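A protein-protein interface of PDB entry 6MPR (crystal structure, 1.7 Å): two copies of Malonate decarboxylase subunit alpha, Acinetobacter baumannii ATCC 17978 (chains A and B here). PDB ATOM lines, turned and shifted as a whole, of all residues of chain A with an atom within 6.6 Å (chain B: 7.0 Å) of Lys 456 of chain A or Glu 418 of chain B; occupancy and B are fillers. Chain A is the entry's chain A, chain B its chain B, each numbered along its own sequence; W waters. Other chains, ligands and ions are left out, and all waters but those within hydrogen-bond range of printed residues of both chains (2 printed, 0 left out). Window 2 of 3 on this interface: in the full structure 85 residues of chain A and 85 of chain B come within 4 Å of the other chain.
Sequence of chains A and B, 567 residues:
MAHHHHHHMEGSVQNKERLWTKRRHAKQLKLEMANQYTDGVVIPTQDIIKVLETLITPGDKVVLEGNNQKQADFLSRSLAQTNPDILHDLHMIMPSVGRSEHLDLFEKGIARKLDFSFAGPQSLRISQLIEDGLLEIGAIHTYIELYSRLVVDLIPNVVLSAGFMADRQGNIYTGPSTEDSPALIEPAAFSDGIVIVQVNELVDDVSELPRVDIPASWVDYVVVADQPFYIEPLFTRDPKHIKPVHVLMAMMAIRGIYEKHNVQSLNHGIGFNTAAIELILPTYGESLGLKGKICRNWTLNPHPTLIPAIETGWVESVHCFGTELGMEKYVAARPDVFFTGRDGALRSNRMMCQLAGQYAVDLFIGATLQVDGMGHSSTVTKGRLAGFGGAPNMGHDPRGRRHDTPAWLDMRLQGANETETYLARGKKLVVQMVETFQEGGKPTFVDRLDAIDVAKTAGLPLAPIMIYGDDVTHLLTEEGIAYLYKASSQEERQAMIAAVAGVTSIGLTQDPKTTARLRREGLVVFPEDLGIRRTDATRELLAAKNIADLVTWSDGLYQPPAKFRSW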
ATOM      1  N   ARG A 448      -5.895 -18.776 -11.090  1.00  0.00           N
ATOM      2  CA  ARG A 448      -6.874 -19.362 -11.996  1.00  0.00           C
ATOM      3  C   ARG A 448      -6.751 -18.709 -13.364  1.00  0.00           C
ATOM      4  O   ARG A 448      -6.845 -17.483 -13.479  1.00  0.00           O
ATOM      5  CB  ARG A 448      -8.297 -19.172 -11.447  1.00  0.00           C
ATOM      6  CG  ARG A 448      -9.427 -19.636 -12.347  1.00  0.00           C
ATOM      7  CD  ARG A 448     -10.763 -19.126 -11.814  1.00  0.00           C
ATOM      8  NE  ARG A 448     -11.907 -19.570 -12.618  1.00  0.00           N
ATOM      9  CZ  ARG A 448     -12.527 -20.730 -12.436  1.00  0.00           C
ATOM     10  NH1 ARG A 448     -12.111 -21.559 -11.480  1.00  0.00           N
ATOM     11  NH2 ARG A 448     -13.557 -21.067 -13.206  1.00  0.00           N
ATOM     12  N   ALA A 451      -8.818 -18.567 -18.977  1.00  0.00           N
ATOM     13  CA  ALA A 451      -9.283 -19.468 -20.025  1.00  0.00           C
ATOM     14  C   ALA A 451     -10.431 -20.347 -19.558  1.00  0.00           C
ATOM     15  O   ALA A 451     -11.296 -20.707 -20.359  1.00  0.00           O
ATOM     16  CB  ALA A 451      -8.125 -20.340 -20.511  1.00  0.00           C
ATOM     17  N   ILE A 452     -10.455 -20.708 -18.272  1.00  0.00           N
ATOM     18  CA  ILE A 452     -11.510 -21.589 -17.774  1.00  0.00           C
ATOM     19  C   ILE A 452     -12.869 -20.929 -17.921  1.00  0.00           C
ATOM     20  O   ILE A 452     -13.812 -21.529 -18.444  1.00  0.00           O
ATOM     21  CB  ILE A 452     -11.251 -21.990 -16.314  1.00  0.00           C
ATOM     22  CG1 ILE A 452      -9.898 -22.697 -16.174  1.00  0.00           C
ATOM     23  CG2 ILE A 452     -12.398 -22.858 -15.838  1.00  0.00           C
ATOM     24  CD1 ILE A 452      -9.428 -22.760 -14.741  1.00  0.00           C
ATOM     25  N   ASP A 453     -12.998 -19.684 -17.452  1.00  0.00           N
ATOM     26  CA  ASP A 453     -14.293 -19.016 -17.586  1.00  0.00           C
ATOM     27  C   ASP A 453     -14.609 -18.662 -19.040  1.00  0.00           C
ATOM     28  O   ASP A 453     -15.788 -18.634 -19.420  1.00  0.00           O
ATOM     29  CB  ASP A 453     -14.350 -17.770 -16.703  1.00  0.00           C
ATOM     30  CG  ASP A 453     -14.611 -18.100 -15.243  1.00  0.00           C
ATOM     31  OD1 ASP A 453     -14.710 -19.299 -14.905  1.00  0.00           O
ATOM     32  OD2 ASP A 453     -14.715 -17.160 -14.428  1.00  0.00           O
ATOM     33  N   VAL A 454     -13.591 -18.393 -19.871  1.00  0.00           N
ATOM     34  CA  VAL A 454     -13.870 -18.166 -21.287  1.00  0.00           C
ATOM     35  C   VAL A 454     -14.467 -19.421 -21.914  1.00  0.00           C
ATOM     36  O   VAL A 454     -15.411 -19.345 -22.708  1.00  0.00           O
ATOM     37  CB  VAL A 454     -12.609 -17.710 -22.042  1.00  0.00           C
ATOM     38  CG1 VAL A 454     -12.890 -17.703 -23.535  1.00  0.00           C
ATOM     39  CG2 VAL A 454     -12.188 -16.317 -21.591  1.00  0.00           C
ATOM     40  N   ALA A 455     -13.939 -20.593 -21.560  1.00  0.00           N
ATOM     41  CA  ALA A 455     -14.513 -21.845 -22.053  1.00  0.00           C
ATOM     42  C   ALA A 455     -15.985 -21.963 -21.673  1.00  0.00           C
ATOM     43  O   ALA A 455     -16.822 -22.337 -22.505  1.00  0.00           O
ATOM     44  CB  ALA A 455     -13.721 -23.040 -21.517  1.00  0.00           C
ATOM     45  N   LYS A 456     -16.323 -21.641 -20.419  1.00  0.00           N
ATOM     46  CA  LYS A 456     -17.720 -21.685 -19.987  1.00  0.00           C
ATOM     47  C   LYS A 456     -18.576 -20.709 -20.781  1.00  0.00           C
ATOM     48  O   LYS A 456     -19.666 -21.059 -21.249  1.00  0.00           O
ATOM     49  CB  LYS A 456     -17.818 -21.375 -18.492  1.00  0.00           C
ATOM     50  CG  LYS A 456     -17.204 -22.441 -17.612  1.00  0.00           C
ATOM     51  CD  LYS A 456     -16.876 -21.930 -16.213  1.00  0.00           C
ATOM     52  CE  LYS A 456     -18.123 -21.677 -15.393  1.00  0.00           C
ATOM     53  NZ  LYS A 456     -17.769 -21.364 -13.979  1.00  0.00           N
ATOM     54  N   THR A 457     -18.098 -19.474 -20.935  1.00  0.00           N
ATOM     55  CA  THR A 457     -18.886 -18.436 -21.594  1.00  0.00           C
ATOM     56  C   THR A 457     -19.090 -18.740 -23.076  1.00  0.00           C
ATOM     57  O   THR A 457     -20.185 -18.521 -23.618  1.00  0.00           O
ATOM     58  CB  THR A 457     -18.195 -17.090 -21.401  1.00  0.00           C
ATOM     59  OG1 THR A 457     -18.151 -16.791 -20.001  1.00  0.00           O
ATOM     60  CG2 THR A 457     -18.931 -15.980 -22.131  1.00  0.00           C
ATOM     61  N   ALA A 458     -18.057 -19.262 -23.741  1.00  0.00           N
ATOM     62  CA  ALA A 458     -18.093 -19.556 -25.165  1.00  0.00           C
ATOM     63  C   ALA A 458     -18.609 -20.951 -25.490  1.00  0.00           C
ATOM     64  O   ALA A 458     -18.756 -21.274 -26.672  1.00  0.00           O
ATOM     65  CB  ALA A 458     -16.697 -19.391 -25.776  1.00  0.00           C
ATOM     66  N   GLY A 459     -18.865 -21.790 -24.489  1.00  0.00           N
ATOM     67  CA  GLY A 459     -19.353 -23.131 -24.752  1.00  0.00           C
ATOM     68  C   GLY A 459     -18.302 -24.121 -25.211  1.00  0.00           C
ATOM     69  O   GLY A 459     -18.614 -25.035 -25.979  1.00  0.00           O
ATOM     70  N   LEU A 460     -17.070 -23.968 -24.771  1.00  0.00           N
ATOM     71  CA  LEU A 460     -16.064 -24.942 -25.166  1.00  0.00           C
ATOM     72  C   LEU A 460     -15.920 -26.015 -24.093  1.00  0.00           C
ATOM     73  O   LEU A 460     -16.050 -25.719 -22.904  1.00  0.00           O
ATOM     74  CB  LEU A 460     -14.704 -24.272 -25.361  1.00  0.00           C
ATOM     75  CG  LEU A 460     -14.665 -23.088 -26.324  1.00  0.00           C
ATOM     76  CD1 LEU A 460     -13.361 -22.329 -26.128  1.00  0.00           C
ATOM     77  CD2 LEU A 460     -14.780 -23.611 -27.740  1.00  0.00           C
ATOM     78  N   LEU A 462     -13.139 -27.665 -23.176  1.00  0.00           N
ATOM     79  CA  LEU A 462     -11.862 -27.549 -22.484  1.00  0.00           C
ATOM     80  C   LEU A 462     -11.482 -26.082 -22.353  1.00  0.00           C
ATOM     81  O   LEU A 462     -11.761 -25.280 -23.246  1.00  0.00           O
ATOM     82  CB  LEU A 462     -10.736 -28.296 -23.233  1.00  0.00           C
ATOM     83  CG  LEU A 462     -10.518 -29.791 -22.969  1.00  0.00           C
ATOM     84  CD1 LEU A 462     -11.656 -30.602 -23.490  1.00  0.00           C
ATOM     85  CD2 LEU A 462      -9.207 -30.253 -23.608  1.00  0.00           C
ATOM     86  N   ARG B 412     -10.998 -38.321 -21.422  1.00  0.00           N
ATOM     87  CA  ARG B 412     -10.650 -37.374 -20.370  1.00  0.00           C
ATOM     88  C   ARG B 412     -11.156 -37.877 -19.024  1.00  0.00           C
ATOM     89  O   ARG B 412     -12.276 -38.378 -18.911  1.00  0.00           O
ATOM     90  CB  ARG B 412     -11.247 -35.998 -20.681  1.00  0.00           C
ATOM     91  CG  ARG B 412     -11.032 -34.958 -19.579  1.00  0.00           C
ATOM     92  CD  ARG B 412     -11.472 -33.549 -19.992  1.00  0.00           C
ATOM     93  NE  ARG B 412     -12.900 -33.453 -20.290  1.00  0.00           N
ATOM     94  CZ  ARG B 412     -13.556 -32.305 -20.437  1.00  0.00           C
ATOM     95  NH1 ARG B 412     -12.912 -31.153 -20.293  1.00  0.00           N
ATOM     96  NH2 ARG B 412     -14.855 -32.308 -20.718  1.00  0.00           N
ATOM     97  N   GLY B 415     -12.530 -34.395 -13.372  1.00  0.00           N
ATOM     98  CA  GLY B 415     -11.807 -33.826 -12.257  1.00  0.00           C
ATOM     99  C   GLY B 415     -12.640 -33.813 -10.990  1.00  0.00           C
ATOM    100  O   GLY B 415     -13.814 -34.187 -10.970  1.00  0.00           O
ATOM    101  N   ALA B 416     -12.003 -33.356  -9.911  1.00  0.00           N
ATOM    102  CA  ALA B 416     -12.681 -33.229  -8.629  1.00  0.00           C
ATOM    103  C   ALA B 416     -13.761 -32.160  -8.640  1.00  0.00           C
ATOM    104  O   ALA B 416     -14.539 -32.083  -7.680  1.00  0.00           O
ATOM    105  CB  ALA B 416     -11.667 -32.926  -7.528  1.00  0.00           C
ATOM    106  N   ASN B 417     -13.835 -31.349  -9.691  1.00  0.00           N
ATOM    107  CA  ASN B 417     -14.820 -30.277  -9.783  1.00  0.00           C
ATOM    108  C   ASN B 417     -14.822 -29.767 -11.222  1.00  0.00           C
ATOM    109  O   ASN B 417     -14.079 -30.255 -12.076  1.00  0.00           O
ATOM    110  CB  ASN B 417     -14.512 -29.168  -8.777  1.00  0.00           C
ATOM    111  CG  ASN B 417     -13.072 -28.689  -8.860  1.00  0.00           C
ATOM    112  OD1 ASN B 417     -12.554 -28.428  -9.944  1.00  0.00           O
ATOM    113  ND2 ASN B 417     -12.418 -28.586  -7.715  1.00  0.00           N
ATOM    114  N   GLU B 418     -15.668 -28.772 -11.478  1.00  0.00           N
ATOM    115  CA  GLU B 418     -15.803 -28.230 -12.825  1.00  0.00           C
ATOM    116  C   GLU B 418     -14.487 -27.641 -13.322  1.00  0.00           C
ATOM    117  O   GLU B 418     -14.095 -27.859 -14.476  1.00  0.00           O
ATOM    118  CB  GLU B 418     -16.904 -27.169 -12.828  1.00  0.00           C
ATOM    119  CG  GLU B 418     -17.170 -26.531 -14.168  1.00  0.00           C
ATOM    120  CD  GLU B 418     -18.137 -25.359 -14.068  1.00  0.00           C
ATOM    121  OE1 GLU B 418     -17.748 -24.293 -13.541  1.00  0.00           O
ATOM    122  OE2 GLU B 418     -19.293 -25.512 -14.512  1.00  0.00           O
ATOM    123  N   THR B 419     -13.797 -26.893 -12.455  1.00  0.00           N
ATOM    124  CA  THR B 419     -12.548 -26.234 -12.827  1.00  0.00           C
ATOM    125  C   THR B 419     -11.496 -27.253 -13.248  1.00  0.00           C
ATOM    126  O   THR B 419     -10.862 -27.110 -14.301  1.00  0.00           O
ATOM    127  CB  THR B 419     -12.054 -25.378 -11.656  1.00  0.00           C
ATOM    128  OG1 THR B 419     -12.953 -24.277 -11.446  1.00  0.00           O
ATOM    129  CG2 THR B 419     -10.652 -24.841 -11.898  1.00  0.00           C
ATOM    130  N   GLU B 420     -11.319 -28.313 -12.453  1.00  0.00           N
ATOM    131  CA  GLU B 420     -10.295 -29.292 -12.800  1.00  0.00           C
ATOM    132  C   GLU B 420     -10.666 -30.082 -14.056  1.00  0.00           C
ATOM    133  O   GLU B 420      -9.775 -30.491 -14.807  1.00  0.00           O
ATOM    134  CB  GLU B 420     -10.031 -30.222 -11.613  1.00  0.00           C
ATOM    135  CG  GLU B 420      -9.463 -29.494 -10.380  1.00  0.00           C
ATOM    136  CD  GLU B 420      -8.286 -28.556 -10.697  1.00  0.00           C
ATOM    137  OE1 GLU B 420      -7.319 -28.991 -11.359  1.00  0.00           O
ATOM    138  OE2 GLU B 420      -8.327 -27.379 -10.276  1.00  0.00           O
ATOM    139  N   THR B 421     -11.959 -30.286 -14.323  1.00  0.00           N
ATOM    140  CA  THR B 421     -12.334 -30.935 -15.577  1.00  0.00           C
ATOM    141  C   THR B 421     -11.984 -30.062 -16.775  1.00  0.00           C
ATOM    142  O   THR B 421     -11.514 -30.571 -17.803  1.00  0.00           O
ATOM    143  CB  THR B 421     -13.828 -31.274 -15.588  1.00  0.00           C
ATOM    144  OG1 THR B 421     -14.116 -32.204 -14.539  1.00  0.00           O
ATOM    145  CG2 THR B 421     -14.208 -31.915 -16.911  1.00  0.00           C
ATOM    146  N   TYR B 422     -12.206 -28.749 -16.664  1.00  0.00           N
ATOM    147  CA  TYR B 422     -11.834 -27.839 -17.749  1.00  0.00           C
ATOM    148  C   TYR B 422     -10.330 -27.838 -18.005  1.00  0.00           C
ATOM    149  O   TYR B 422      -9.895 -27.622 -19.146  1.00  0.00           O
ATOM    150  CB  TYR B 422     -12.303 -26.417 -17.439  1.00  0.00           C
ATOM    151  CG  TYR B 422     -13.746 -26.157 -17.818  1.00  0.00           C
ATOM    152  CD1 TYR B 422     -14.157 -26.250 -19.139  1.00  0.00           C
ATOM    153  CD2 TYR B 422     -14.687 -25.815 -16.863  1.00  0.00           C
ATOM    154  CE1 TYR B 422     -15.469 -26.006 -19.507  1.00  0.00           C
ATOM    155  CE2 TYR B 422     -16.002 -25.576 -17.216  1.00  0.00           C
ATOM    156  CZ  TYR B 422     -16.387 -25.673 -18.544  1.00  0.00           C
ATOM    157  OH  TYR B 422     -17.703 -25.430 -18.903  1.00  0.00           O
ATOM    158  N   LEU B 423      -9.519 -28.060 -16.969  1.00  0.00           N
ATOM    159  CA  LEU B 423      -8.071 -28.132 -17.155  1.00  0.00           C
ATOM    160  C   LEU B 423      -7.594 -29.506 -17.592  1.00  0.00           C
ATOM    161  O   LEU B 423      -6.408 -29.659 -17.908  1.00  0.00           O
ATOM    162  CB  LEU B 423      -7.342 -27.735 -15.860  1.00  0.00           C
ATOM    163  CG  LEU B 423      -7.614 -26.299 -15.437  1.00  0.00           C
ATOM    164  CD1 LEU B 423      -7.165 -26.052 -14.015  1.00  0.00           C
ATOM    165  CD2 LEU B 423      -6.939 -25.352 -16.421  1.00  0.00           C
ATOM    166  N   ALA B 424      -8.477 -30.503 -17.615  1.00  0.00           N
ATOM    167  CA  ALA B 424      -8.122 -31.844 -18.040  1.00  0.00           C
ATOM    168  C   ALA B 424      -8.244 -31.942 -19.550  1.00  0.00           C
ATOM    169  O   ALA B 424      -8.966 -31.175 -20.187  1.00  0.00           O
ATOM    170  CB  ALA B 424      -9.025 -32.884 -17.369  1.00  0.00           C
HETATM  171  O   HOH W   1     -15.035 -23.874 -13.349  1.00  0.00           O
HETATM  172  O   HOH W   2     -18.268 -25.275 -21.522  1.00  0.00           O
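Water W2 lies within hydrogen-bond range of the backbone carbonyl oxygen (O) of Leu 460 of chain A (2.7 Å), the side-chain hydroxyl (OH) of Tyr 422 of chain B (2.7 Å) and the backbone carbonyl oxygen (O) of Ala 455 of chain A (3.4 Å). Water W1 lies within hydrogen-bond range of OE1 of Glu 418 of chain B, OG1 of Thr 419 of chain B and NH2 of Arg 448 of chain A.
Of the 11 printed residues of chain B, 6 touch a printed residue of chain A. Hydrophobic or aromatic side chains of chain B that line the printed part of chain A: Tyr 422 and Leu 423. Of the 12 printed residues of chain A, 6 touch a printed residue of chain B. Among the printed residues, Asp or Glu carboxylates within 4 Å of a Lys or Arg side-chain nitrogen of the other chain: Lys 456 of chain A with Glu 418 of chain B (3.0 Å).
The side-chain amino group (NZ) of Lys 456 of chain A is in salt-bridge range of the side-chain carboxylate (OE1) of Glu 418 of chain B, at 3.0 Å. OG1 of Thr 419 of chain B sits at hydrogen-bond distance from NH1 of Arg 448 of chain A (2.8 Å).
CD1 of Ile 452 of chain A touches CG2 of Thr 419 of chain B, at 3.7 Å. Ile 452 of chain A touches Tyr 422 of chain B (CG2 to CD2, 3.9 Å). CD1 of Ile 452 of chain A touches CD2 of Leu 423 of chain B, at 3.97 Å. Ala 455 of chain A touches Tyr 422 of chain B. Tyr 422 of chain B touches Lys 456 of chain A (OH to CG, 3.3 Å). O of Leu 460 of chain A touches CE1 of Tyr 422 of chain B (3.5 Å). Arg 412 of chain B touches Leu 462 of chain A (NH1 to CD1, 3.5 Å). Leu 462 of chain A touches Tyr 422 of chain B (CA to O, 3.9 Å). Leu 462 of chain A touches Ala 424 of chain B.
The guanidinium group (NH2) of Arg 448 of chain A is in salt-bridge range of the side-chain carboxylate (OD1) of Asp 453 of chain A (2.7 Å). The backbone carbonyl oxygen (O) of Ala 455 of chain A sits at hydrogen-bond distance from the backbone NH (N) of Leu 460 of chain A, 2.8 Å away. N of Thr 419 of chain B is in hydrogen-bond range of OD1 of Asn 417 of chain B, at 3.2 Å. OD1 of Asp 453 of chain A lies within salt-bridge range of NZ of Lys 456 of chain A, 3.8 Å away. NH1 of Arg 412 of chain B sits at hydrogen-bond distance from O of Thr 421 of chain B (2.9 Å).
Of chain B, only Glu 418 (3.0 Å) and Tyr 422 (3.3 Å) come within 4 Å of Lys 456 of chain A. Ala 458 of chain A touches none of the printed residues of chain B. Of the printed residues of chain A, Thr 419 of chain B touches Arg 448 and Ile 452. Of the printed residues of chain A, Leu 423 of chain B touches Ile 452. The nearest residue of chain A that does not touch Glu 418 of chain B is Arg 448 of chain A (5.3 Å).
No position is printed for both chains. Of the 11 pairs that touch across the chains among the printed residues, none has its exchanged pair printed and touching as well.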
